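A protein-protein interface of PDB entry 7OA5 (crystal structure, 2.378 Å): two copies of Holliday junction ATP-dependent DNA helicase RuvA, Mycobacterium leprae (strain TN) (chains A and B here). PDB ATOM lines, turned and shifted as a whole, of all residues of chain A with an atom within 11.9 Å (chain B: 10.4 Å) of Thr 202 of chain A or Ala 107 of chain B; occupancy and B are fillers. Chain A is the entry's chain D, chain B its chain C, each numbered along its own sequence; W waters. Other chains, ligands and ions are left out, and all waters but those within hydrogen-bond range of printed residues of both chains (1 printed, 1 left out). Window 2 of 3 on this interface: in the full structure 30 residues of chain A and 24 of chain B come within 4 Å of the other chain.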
ATOM      1  N   PHE A 163      25.373 -25.870  40.220  1.00  0.00           N
ATOM      2  CA  PHE A 163      26.631 -25.211  40.536  1.00  0.00           C
ATOM      3  C   PHE A 163      27.240 -25.769  41.806  1.00  0.00           C
ATOM      4  O   PHE A 163      26.514 -26.163  42.727  1.00  0.00           O
ATOM      5  CB  PHE A 163      26.462 -23.689  40.650  1.00  0.00           C
ATOM      6  CG  PHE A 163      26.238 -22.993  39.332  1.00  0.00           C
ATOM      7  CD1 PHE A 163      27.305 -22.684  38.502  1.00  0.00           C
ATOM      8  CD2 PHE A 163      24.964 -22.652  38.917  1.00  0.00           C
ATOM      9  CE1 PHE A 163      27.094 -22.055  37.284  1.00  0.00           C
ATOM     10  CE2 PHE A 163      24.761 -22.016  37.709  1.00  0.00           C
ATOM     11  CZ  PHE A 163      25.828 -21.702  36.909  1.00  0.00           C
ATOM     12  N   GLN A 167      31.565 -22.221  44.053  1.00  0.00           N
ATOM     13  CA  GLN A 167      31.326 -21.337  42.903  1.00  0.00           C
ATOM     14  C   GLN A 167      29.996 -20.548  43.072  1.00  0.00           C
ATOM     15  O   GLN A 167      29.906 -19.394  42.655  1.00  0.00           O
ATOM     16  CB  GLN A 167      31.335 -22.126  41.579  1.00  0.00           C
ATOM     17  CG  GLN A 167      32.429 -21.714  40.582  1.00  0.00           C
ATOM     18  CD  GLN A 167      32.298 -20.333  39.938  1.00  0.00           C
ATOM     19  OE1 GLN A 167      32.212 -19.280  40.614  1.00  0.00           O
ATOM     20  NE2 GLN A 167      32.364 -20.303  38.598  1.00  0.00           N
ATOM     21  N   GLN A 174      29.992 -11.912  45.187  1.00  0.00           N
ATOM     22  CA  GLN A 174      30.402 -10.864  44.250  1.00  0.00           C
ATOM     23  C   GLN A 174      29.224  -9.936  43.869  1.00  0.00           C
ATOM     24  O   GLN A 174      29.423  -8.764  43.573  1.00  0.00           O
ATOM     25  CB  GLN A 174      31.030 -11.489  42.997  1.00  0.00           C
ATOM     26  CG  GLN A 174      31.467 -10.455  41.965  1.00  0.00           C
ATOM     27  CD  GLN A 174      32.299 -11.028  40.854  1.00  0.00           C
ATOM     28  OE1 GLN A 174      32.784 -12.173  40.916  1.00  0.00           O
ATOM     29  NE2 GLN A 174      32.475 -10.232  39.801  1.00  0.00           N
ATOM     30  N   ALA A 194      21.443 -11.976  38.754  1.00  0.00           N
ATOM     31  CA  ALA A 194      22.755 -11.320  38.708  1.00  0.00           C
ATOM     32  C   ALA A 194      23.883 -12.354  38.907  1.00  0.00           C
ATOM     33  O   ALA A 194      24.893 -12.297  38.215  1.00  0.00           O
ATOM     34  CB  ALA A 194      22.835 -10.250  39.788  1.00  0.00           C
ATOM     35  N   ALA A 195      23.708 -13.311  39.845  1.00  0.00           N
ATOM     36  CA  ALA A 195      24.705 -14.357  40.066  1.00  0.00           C
ATOM     37  C   ALA A 195      24.818 -15.276  38.846  1.00  0.00           C
ATOM     38  O   ALA A 195      25.925 -15.618  38.443  1.00  0.00           O
ATOM     39  CB  ALA A 195      24.365 -15.163  41.310  1.00  0.00           C
ATOM     40  N   LEU A 196      23.682 -15.614  38.216  1.00  0.00           N
ATOM     41  CA  LEU A 196      23.647 -16.442  37.016  1.00  0.00           C
ATOM     42  C   LEU A 196      24.250 -15.729  35.813  1.00  0.00           C
ATOM     43  O   LEU A 196      24.865 -16.373  34.945  1.00  0.00           O
ATOM     44  CB  LEU A 196      22.213 -16.865  36.708  1.00  0.00           C
ATOM     45  CG  LEU A 196      21.705 -17.973  37.597  1.00  0.00           C
ATOM     46  CD1 LEU A 196      20.188 -18.063  37.536  1.00  0.00           C
ATOM     47  CD2 LEU A 196      22.334 -19.298  37.214  1.00  0.00           C
ATOM     48  N   SER A 197      24.045 -14.406  35.734  1.00  0.00           N
ATOM     49  CA  SER A 197      24.604 -13.591  34.660  1.00  0.00           C
ATOM     50  C   SER A 197      26.139 -13.616  34.759  1.00  0.00           C
ATOM     51  O   SER A 197      26.833 -13.815  33.760  1.00  0.00           O
ATOM     52  CB  SER A 197      24.097 -12.159  34.783  1.00  0.00           C
ATOM     53  OG  SER A 197      24.695 -11.321  33.812  1.00  0.00           O
ATOM     54  N   LEU A 198      26.650 -13.473  35.979  1.00  0.00           N
ATOM     55  CA  LEU A 198      28.060 -13.520  36.275  1.00  0.00           C
ATOM     56  C   LEU A 198      28.645 -14.915  35.989  1.00  0.00           C
ATOM     57  O   LEU A 198      29.690 -15.017  35.349  1.00  0.00           O
ATOM     58  CB  LEU A 198      28.217 -13.148  37.749  1.00  0.00           C
ATOM     59  CG  LEU A 198      29.573 -13.253  38.346  1.00  0.00           C
ATOM     60  CD1 LEU A 198      30.590 -12.357  37.575  1.00  0.00           C
ATOM     61  CD2 LEU A 198      29.506 -12.857  39.816  1.00  0.00           C
ATOM     62  N   LEU A 199      27.950 -15.988  36.402  1.00  0.00           N
ATOM     63  CA  LEU A 199      28.408 -17.364  36.186  1.00  0.00           C
ATOM     64  C   LEU A 199      28.475 -17.779  34.721  1.00  0.00           C
ATOM     65  O   LEU A 199      29.251 -18.672  34.378  1.00  0.00           O
ATOM     66  CB  LEU A 199      27.558 -18.352  36.996  1.00  0.00           C
ATOM     67  CG  LEU A 199      27.837 -18.308  38.481  1.00  0.00           C
ATOM     68  CD1 LEU A 199      26.690 -18.854  39.303  1.00  0.00           C
ATOM     69  CD2 LEU A 199      29.098 -19.022  38.792  1.00  0.00           C
ATOM     70  N   GLY A 200      27.682 -17.143  33.870  1.00  0.00           N
ATOM     71  CA  GLY A 200      27.689 -17.453  32.446  1.00  0.00           C
ATOM     72  C   GLY A 200      28.723 -16.696  31.633  1.00  0.00           C
ATOM     73  O   GLY A 200      28.820 -16.894  30.420  1.00  0.00           O
ATOM     74  N   LYS A 201      29.483 -15.786  32.281  1.00  0.00           N
ATOM     75  CA  LYS A 201      30.560 -15.031  31.642  1.00  0.00           C
ATOM     76  C   LYS A 201      31.676 -16.037  31.340  1.00  0.00           C
ATOM     77  O   LYS A 201      32.095 -16.789  32.238  1.00  0.00           O
ATOM     78  CB  LYS A 201      31.107 -13.929  32.572  1.00  0.00           C
ATOM     79  CG  LYS A 201      30.432 -12.582  32.446  1.00  0.00           C
ATOM     80  N   THR A 202      32.117 -16.083  30.072  1.00  0.00           N
ATOM     81  CA  THR A 202      33.162 -17.011  29.625  1.00  0.00           C
ATOM     82  C   THR A 202      34.517 -16.777  30.361  1.00  0.00           C
ATOM     83  O   THR A 202      35.341 -17.694  30.459  1.00  0.00           O
ATOM     84  CB  THR A 202      33.262 -16.970  28.095  1.00  0.00           C
ATOM     85  OG1 THR A 202      33.706 -18.237  27.600  1.00  0.00           O
ATOM     86  CG2 THR A 202      34.123 -15.811  27.588  1.00  0.00           C
ATOM     87  N   ARG A 203      34.705 -15.580  30.946  1.00  0.00           N
ATOM     88  CA  ARG A 203      35.883 -15.242  31.734  1.00  0.00           C
ATOM     89  C   ARG A 203      35.875 -16.034  33.058  1.00  0.00           C
ATOM     90  O   ARG A 203      35.959 -17.267  33.053  1.00  0.00           O
ATOM     91  CB  ARG A 203      35.899 -13.728  32.021  1.00  0.00           C
ATOM     92  N   VAL B  91      21.420 -20.025  32.570  1.00  0.00           N
ATOM     93  CA  VAL B  91      22.726 -19.419  32.402  1.00  0.00           C
ATOM     94  C   VAL B  91      22.780 -18.582  31.115  1.00  0.00           C
ATOM     95  O   VAL B  91      23.285 -17.462  31.136  1.00  0.00           O
ATOM     96  CB  VAL B  91      23.817 -20.526  32.448  1.00  0.00           C
ATOM     97  CG1 VAL B  91      25.182 -20.002  32.012  1.00  0.00           C
ATOM     98  CG2 VAL B  91      23.889 -21.171  33.828  1.00  0.00           C
ATOM     99  N   HIS B  92      22.237 -19.094  30.019  1.00  0.00           N
ATOM    100  CA  HIS B  92      22.264 -18.380  28.756  1.00  0.00           C
ATOM    101  C   HIS B  92      20.900 -17.924  28.280  1.00  0.00           C
ATOM    102  O   HIS B  92      19.965 -18.730  28.185  1.00  0.00           O
ATOM    103  CB  HIS B  92      22.961 -19.198  27.652  1.00  0.00           C
ATOM    104  CG  HIS B  92      24.347 -19.605  28.017  1.00  0.00           C
ATOM    105  ND1 HIS B  92      25.324 -18.660  28.311  1.00  0.00           N
ATOM    106  CD2 HIS B  92      24.871 -20.840  28.176  1.00  0.00           C
ATOM    107  CE1 HIS B  92      26.404 -19.354  28.629  1.00  0.00           C
ATOM    108  NE2 HIS B  92      26.183 -20.668  28.547  1.00  0.00           N
ATOM    109  N   ALA B  96      22.063 -15.425  23.382  1.00  0.00           N
ATOM    110  CA  ALA B  96      23.399 -15.913  23.719  1.00  0.00           C
ATOM    111  C   ALA B  96      23.567 -17.391  23.370  1.00  0.00           C
ATOM    112  O   ALA B  96      24.601 -17.775  22.838  1.00  0.00           O
ATOM    113  CB  ALA B  96      23.688 -15.690  25.191  1.00  0.00           C
ATOM    114  N   LEU B  97      22.544 -18.203  23.633  1.00  0.00           N
ATOM    115  CA  LEU B  97      22.567 -19.625  23.343  1.00  0.00           C
ATOM    116  C   LEU B  97      22.557 -19.879  21.840  1.00  0.00           C
ATOM    117  O   LEU B  97      23.332 -20.693  21.355  1.00  0.00           O
ATOM    118  CB  LEU B  97      21.373 -20.321  24.019  1.00  0.00           C
ATOM    119  CG  LEU B  97      21.300 -21.823  23.832  1.00  0.00           C
ATOM    120  CD1 LEU B  97      22.486 -22.491  24.448  1.00  0.00           C
ATOM    121  CD2 LEU B  97      20.018 -22.382  24.435  1.00  0.00           C
ATOM    122  N   GLN B  99      23.645 -17.892  19.577  1.00  0.00           N
ATOM    123  CA  GLN B  99      24.928 -17.397  19.125  1.00  0.00           C
ATOM    124  C   GLN B  99      25.976 -18.485  19.371  1.00  0.00           C
ATOM    125  O   GLN B  99      26.695 -18.851  18.443  1.00  0.00           O
ATOM    126  CB  GLN B  99      25.273 -16.100  19.885  1.00  0.00           C
ATOM    127  CG  GLN B  99      26.698 -15.612  19.694  1.00  0.00           C
ATOM    128  CD  GLN B  99      26.809 -14.530  18.651  1.00  0.00           C
ATOM    129  OE1 GLN B  99      25.943 -14.369  17.773  1.00  0.00           O
ATOM    130  NE2 GLN B  99      27.893 -13.769  18.724  1.00  0.00           N
ATOM    131  N   ALA B 100      26.018 -19.043  20.594  1.00  0.00           N
ATOM    132  CA  ALA B 100      26.958 -20.086  20.953  1.00  0.00           C
ATOM    133  C   ALA B 100      26.839 -21.318  20.058  1.00  0.00           C
ATOM    134  O   ALA B 100      27.829 -21.995  19.843  1.00  0.00           O
ATOM    135  CB  ALA B 100      26.776 -20.472  22.405  1.00  0.00           C
ATOM    136  N   LEU B 101      25.653 -21.594  19.515  1.00  0.00           N
ATOM    137  CA  LEU B 101      25.460 -22.737  18.632  1.00  0.00           C
ATOM    138  C   LEU B 101      26.039 -22.429  17.258  1.00  0.00           C
ATOM    139  O   LEU B 101      26.802 -23.232  16.716  1.00  0.00           O
ATOM    140  CB  LEU B 101      23.975 -23.122  18.554  1.00  0.00           C
ATOM    141  CG  LEU B 101      23.374 -23.591  19.885  1.00  0.00           C
ATOM    142  CD1 LEU B 101      21.872 -23.719  19.800  1.00  0.00           C
ATOM    143  CD2 LEU B 101      24.023 -24.877  20.363  1.00  0.00           C
ATOM    144  N   ASP B 103      28.384 -20.131  16.466  1.00  0.00           N
ATOM    145  CA  ASP B 103      29.829 -19.987  16.578  1.00  0.00           C
ATOM    146  C   ASP B 103      30.526 -21.211  17.164  1.00  0.00           C
ATOM    147  O   ASP B 103      31.721 -21.119  17.450  1.00  0.00           O
ATOM    148  CB  ASP B 103      30.175 -18.788  17.474  1.00  0.00           C
ATOM    149  CG  ASP B 103      29.680 -17.450  16.970  1.00  0.00           C
ATOM    150  OD1 ASP B 103      29.300 -17.367  15.771  1.00  0.00           O
ATOM    151  OD2 ASP B 103      29.661 -16.485  17.776  1.00  0.00           O
ATOM    152  N   SER B 104      29.797 -22.321  17.433  1.00  0.00           N
ATOM    153  CA  SER B 104      30.361 -23.537  18.043  1.00  0.00           C
ATOM    154  C   SER B 104      31.149 -23.220  19.313  1.00  0.00           C
ATOM    155  O   SER B 104      32.209 -23.793  19.553  1.00  0.00           O
ATOM    156  CB  SER B 104      31.223 -24.305  17.045  1.00  0.00           C
ATOM    157  OG  SER B 104      30.501 -24.511  15.842  1.00  0.00           O
ATOM    158  N   ASP B 105      30.628 -22.279  20.102  1.00  0.00           N
ATOM    159  CA  ASP B 105      31.249 -21.790  21.318  1.00  0.00           C
ATOM    160  C   ASP B 105      31.039 -22.766  22.454  1.00  0.00           C
ATOM    161  O   ASP B 105      30.244 -22.528  23.374  1.00  0.00           O
ATOM    162  CB  ASP B 105      30.744 -20.378  21.653  1.00  0.00           C
ATOM    163  CG  ASP B 105      31.510 -19.652  22.740  1.00  0.00           C
ATOM    164  OD1 ASP B 105      32.491 -20.226  23.266  1.00  0.00           O
ATOM    165  OD2 ASP B 105      31.121 -18.514  23.075  1.00  0.00           O
ATOM    166  N   VAL B 106      31.812 -23.850  22.403  1.00  0.00           N
ATOM    167  CA  VAL B 106      31.832 -24.919  23.385  1.00  0.00           C
ATOM    168  C   VAL B 106      32.181 -24.383  24.773  1.00  0.00           C
ATOM    169  O   VAL B 106      31.645 -24.860  25.765  1.00  0.00           O
ATOM    170  CB  VAL B 106      32.815 -26.011  22.892  1.00  0.00           C
ATOM    171  CG1 VAL B 106      33.132 -27.023  23.982  1.00  0.00           C
ATOM    172  CG2 VAL B 106      32.261 -26.703  21.653  1.00  0.00           C
ATOM    173  N   ALA B 107      33.028 -23.348  24.839  1.00  0.00           N
ATOM    174  CA  ALA B 107      33.452 -22.728  26.089  1.00  0.00           C
ATOM    175  C   ALA B 107      32.315 -22.076  26.883  1.00  0.00           C
ATOM    176  O   ALA B 107      32.304 -22.177  28.114  1.00  0.00           O
ATOM    177  CB  ALA B 107      34.547 -21.715  25.817  1.00  0.00           C
ATOM    178  N   SER B 108      31.381 -21.395  26.198  1.00  0.00           N
ATOM    179  CA  SER B 108      30.264 -20.762  26.897  1.00  0.00           C
ATOM    180  C   SER B 108      29.247 -21.814  27.326  1.00  0.00           C
ATOM    181  O   SER B 108      28.762 -21.744  28.460  1.00  0.00           O
ATOM    182  CB  SER B 108      29.630 -19.636  26.078  1.00  0.00           C
ATOM    183  OG  SER B 108      28.870 -20.118  24.983  1.00  0.00           O
ATOM    184  N   LEU B 109      28.997 -22.839  26.471  1.00  0.00           N
ATOM    185  CA  LEU B 109      28.119 -23.959  26.819  1.00  0.00           C
ATOM    186  C   LEU B 109      28.653 -24.710  28.033  1.00  0.00           C
ATOM    187  O   LEU B 109      27.856 -25.075  28.883  1.00  0.00           O
ATOM    188  CB  LEU B 109      27.928 -24.918  25.645  1.00  0.00           C
ATOM    189  CG  LEU B 109      27.019 -24.409  24.551  1.00  0.00           C
ATOM    190  CD1 LEU B 109      27.054 -25.324  23.360  1.00  0.00           C
ATOM    191  CD2 LEU B 109      25.592 -24.278  25.056  1.00  0.00           C
ATOM    192  N   THR B 110      29.995 -24.879  28.176  1.00  0.00           N
ATOM    193  CA  THR B 110      30.533 -25.539  29.377  1.00  0.00           C
ATOM    194  C   THR B 110      30.402 -24.692  30.633  1.00  0.00           C
ATOM    195  O   THR B 110      30.620 -25.221  31.726  1.00  0.00           O
ATOM    196  CB  THR B 110      31.965 -26.070  29.224  1.00  0.00           C
ATOM    197  OG1 THR B 110      32.878 -24.983  29.216  1.00  0.00           O
ATOM    198  CG2 THR B 110      32.132 -26.957  28.018  1.00  0.00           C
ATOM    199  N   ARG B 111      30.037 -23.401  30.517  1.00  0.00           N
ATOM    200  CA  ARG B 111      29.759 -22.593  31.709  1.00  0.00           C
ATOM    201  C   ARG B 111      28.497 -23.136  32.430  1.00  0.00           C
ATOM    202  O   ARG B 111      28.353 -22.947  33.635  1.00  0.00           O
ATOM    203  CB  ARG B 111      29.575 -21.099  31.359  1.00  0.00           C
ATOM    204  CG  ARG B 111      30.836 -20.389  30.840  1.00  0.00           C
ATOM    205  CD  ARG B 111      32.042 -20.509  31.756  1.00  0.00           C
ATOM    206  NE  ARG B 111      31.748 -20.183  33.153  1.00  0.00           N
ATOM    207  CZ  ARG B 111      32.650 -19.743  34.030  1.00  0.00           C
ATOM    208  NH1 ARG B 111      32.291 -19.471  35.282  1.00  0.00           N
ATOM    209  NH2 ARG B 111      33.908 -19.536  33.654  1.00  0.00           N
ATOM    210  N   VAL B 112      27.590 -23.820  31.698  1.00  0.00           N
ATOM    211  CA  VAL B 112      26.404 -24.410  32.280  1.00  0.00           C
ATOM    212  C   VAL B 112      26.832 -25.616  33.090  1.00  0.00           C
ATOM    213  O   VAL B 112      27.491 -26.500  32.556  1.00  0.00           O
ATOM    214  CB  VAL B 112      25.442 -24.838  31.165  1.00  0.00           C
ATOM    215  CG1 VAL B 112      24.250 -25.594  31.740  1.00  0.00           C
ATOM    216  CG2 VAL B 112      25.009 -23.644  30.334  1.00  0.00           C
ATOM    217  N   PRO B 113      26.508 -25.662  34.386  1.00  0.00           N
ATOM    218  CA  PRO B 113      26.896 -26.825  35.194  1.00  0.00           C
ATOM    219  C   PRO B 113      26.180 -28.082  34.727  1.00  0.00           C
ATOM    220  O   PRO B 113      24.999 -28.038  34.391  1.00  0.00           O
ATOM    221  CB  PRO B 113      26.522 -26.420  36.608  1.00  0.00           C
ATOM    222  CG  PRO B 113      25.477 -25.386  36.455  1.00  0.00           C
ATOM    223  CD  PRO B 113      25.693 -24.703  35.148  1.00  0.00           C
ATOM    224  N   ILE B 115      27.155 -29.559  31.980  1.00  0.00           N
ATOM    225  CA  ILE B 115      27.603 -29.629  30.602  1.00  0.00           C
ATOM    226  C   ILE B 115      29.109 -29.462  30.588  1.00  0.00           C
ATOM    227  O   ILE B 115      29.628 -28.396  30.971  1.00  0.00           O
ATOM    228  CB  ILE B 115      26.950 -28.550  29.735  1.00  0.00           C
ATOM    229  CG1 ILE B 115      25.428 -28.713  29.740  1.00  0.00           C
ATOM    230  CG2 ILE B 115      27.549 -28.586  28.319  1.00  0.00           C
ATOM    231  CD1 ILE B 115      24.704 -27.825  28.786  1.00  0.00           C
ATOM    232  N   GLY B 116      29.791 -30.532  30.192  1.00  0.00           N
ATOM    233  CA  GLY B 116      31.242 -30.562  30.048  1.00  0.00           C
ATOM    234  C   GLY B 116      31.623 -30.434  28.594  1.00  0.00           C
ATOM    235  O   GLY B 116      30.755 -30.214  27.746  1.00  0.00           O
ATOM    236  N   LYS B 117      32.908 -30.568  28.275  1.00  0.00           N
ATOM    237  CA  LYS B 117      33.376 -30.443  26.893  1.00  0.00           C
ATOM    238  C   LYS B 117      32.654 -31.378  25.922  1.00  0.00           C
ATOM    239  O   LYS B 117      32.256 -30.956  24.837  1.00  0.00           O
ATOM    240  CB  LYS B 117      34.907 -30.643  26.811  1.00  0.00           C
ATOM    241  N   ARG B 118      32.442 -32.628  26.331  1.00  0.00           N
ATOM    242  CA  ARG B 118      31.784 -33.624  25.485  1.00  0.00           C
ATOM    243  C   ARG B 118      30.325 -33.288  25.227  1.00  0.00           C
ATOM    244  O   ARG B 118      29.883 -33.295  24.081  1.00  0.00           O
ATOM    245  CB  ARG B 118      31.938 -35.038  26.085  1.00  0.00           C
ATOM    246  N   GLY B 119      29.604 -32.956  26.288  1.00  0.00           N
ATOM    247  CA  GLY B 119      28.211 -32.542  26.202  1.00  0.00           C
ATOM    248  C   GLY B 119      28.032 -31.303  25.348  1.00  0.00           C
ATOM    249  O   GLY B 119      27.170 -31.286  24.467  1.00  0.00           O
ATOM    250  N   ALA B 120      28.908 -30.286  25.538  1.00  0.00           N
ATOM    251  CA  ALA B 120      28.855 -29.054  24.756  1.00  0.00           C
ATOM    252  C   ALA B 120      29.070 -29.337  23.281  1.00  0.00           C
ATOM    253  O   ALA B 120      28.365 -28.780  22.443  1.00  0.00           O
ATOM    254  CB  ALA B 120      29.888 -28.064  25.258  1.00  0.00           C
ATOM    255  N   GLU B 121      29.993 -30.250  22.959  1.00  0.00           N
ATOM    256  CA  GLU B 121      30.255 -30.634  21.574  1.00  0.00           C
ATOM    257  C   GLU B 121      29.101 -31.400  20.952  1.00  0.00           C
ATOM    258  O   GLU B 121      28.834 -31.234  19.765  1.00  0.00           O
ATOM    259  CB  GLU B 121      31.553 -31.421  21.469  1.00  0.00           C
ATOM    260  CG  GLU B 121      32.777 -30.559  21.711  1.00  0.00           C
ATOM    261  CD  GLU B 121      34.086 -31.258  21.418  1.00  0.00           C
ATOM    262  OE1 GLU B 121      34.554 -32.049  22.272  1.00  0.00           O
ATOM    263  OE2 GLU B 121      34.645 -31.004  20.326  1.00  0.00           O
ATOM    264  N   ILE B 123      25.848 -30.982  21.846  1.00  0.00           N
ATOM    265  CA  ILE B 123      24.816 -29.963  21.673  1.00  0.00           C
ATOM    266  C   ILE B 123      25.089 -29.160  20.413  1.00  0.00           C
ATOM    267  O   ILE B 123      24.197 -29.047  19.584  1.00  0.00           O
ATOM    268  CB  ILE B 123      24.709 -29.054  22.922  1.00  0.00           C
ATOM    269  CG1 ILE B 123      24.219 -29.856  24.136  1.00  0.00           C
ATOM    270  CG2 ILE B 123      23.828 -27.830  22.659  1.00  0.00           C
ATOM    271  CD1 ILE B 123      24.428 -29.162  25.402  1.00  0.00           C
ATOM    272  N   VAL B 124      26.330 -28.645  20.247  1.00  0.00           N
ATOM    273  CA  VAL B 124      26.745 -27.890  19.063  1.00  0.00           C
ATOM    274  C   VAL B 124      26.564 -28.742  17.814  1.00  0.00           C
ATOM    275  O   VAL B 124      26.003 -28.268  16.825  1.00  0.00           O
ATOM    276  CB  VAL B 124      28.207 -27.401  19.188  1.00  0.00           C
ATOM    277  CG1 VAL B 124      28.745 -26.909  17.851  1.00  0.00           C
ATOM    278  CG2 VAL B 124      28.322 -26.305  20.237  1.00  0.00           C
HETATM  279  O   HOH W   1      32.289 -16.512  35.268  1.00  0.00           O
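Phe 163 of chain A touches Val 91 of chain B (CZ to CG2, 3.7 Å).
Phe 163 of chain A touches Arg 111 of chain B (CE1 to O, 3.96 Å).
CZ of Phe 163 of chain A touches CD of Pro 113 of chain B, 3.5 Å away.
CA of Gly 200 of chain A touches CG1 of Val 91 of chain B, 3.6 Å away.
His 92 of chain B touches Gly 200 of chain A.
CZ of Arg 111 of chain B touches O of Lys 201 of chain A, at 3.5 Å.
OG1 of Thr 202 of chain A touches CB of Ala 107 of chain B, 3.998 Å away.
Thr 202 of chain A touches Arg 111 of chain B.
Printed residues of chain B within 4 Å of Thr 202 of chain A: Ala 107 (3.998 Å) and Arg 111 (3.96 Å).
Printed residues of chain A within 4 Å of Ala 107 of chain B: Thr 202.
Gly 200 of chain A touches two residues of chain B.
Lys 201 of chain A touches just one residue of chain B: Arg 111.
Arg 203 of chain A touches one residue of chain B.
No residue of chain A comes within 4 Å of Asp 105 of chain B.
No residue of chain A comes within 4 Å of Val 106 of chain B.
No residue of chain A comes within 4 Å of Thr 110 of chain B.
Of chain A, only Phe 163, Gln 167, Leu 199, Lys 201, Thr 202 and Arg 203 come within 4 Å of Arg 111 of chain B.
Of the printed residues of chain A, Val 91 of chain B touches Phe 163 (3.7 Å) and Gly 200 (3.6 Å).
Of the printed residues of chain A, His 92 of chain B touches Gly 200 (3.9 Å).
Printed residues of chain B within 4 Å of Phe 163 of chain A: Val 91 (3.7 Å), Arg 111 (3.96 Å) and Pro 113 (3.5 Å).
Ser 104 of chain B touches none of the printed residues of chain A.
The nearest printed residue of chain B that does not touch Thr 202 of chain A is Ser 108 of chain B (4.2 Å).
The nearest printed residue of chain A that does not touch Ala 107 of chain B is Gly 200 of chain A (6.7 Å).
Of the 13 printed residues of chain A, 7 touch a printed residue of chain B.
Of the 27 printed residues of chain B, 5 touch a printed residue of chain A.
Printed residues of chain B that touch a printed residue of chain A: Val 91, His 92, Ala 107, Arg 111 and Pro 113.
Among the printed residues, 11 pairs touch across the chains.
No position is printed for both chains.
A ring nitrogen (NE2) of His 92 of chain B is in hydrogen-bond range of the backbone carbonyl oxygen of Ser 108 of chain B, 2.8 Å away.
The side-chain hydroxyl (OG1) of Thr 110 of chain B is in hydrogen-bond range of the backbone carbonyl oxygen (O) of Ala 107 of chain B (3.1 Å).
Water W1 lies within hydrogen-bond range of the guanidinium group of Arg 111 of chain B (3.0 Å), the backbone carbonyl oxygen of Leu 198 of chain A (3.0 Å) and the backbone carbonyl oxygen of Lys 201 of chain A (3.0 Å).
O of Leu 199 of chain A lies within hydrogen-bond range of NE of Arg 111 of chain B (3.2 Å).
NH1 of Arg 111 of chain B sits close to NE2 of Gln 167 of chain A, at 3.4 Å.
The guanidinium group (NH2) of Arg 111 of chain B sits at hydrogen-bond distance from the backbone carbonyl oxygen (O) of Arg 203 of chain A, at 3.1 Å.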
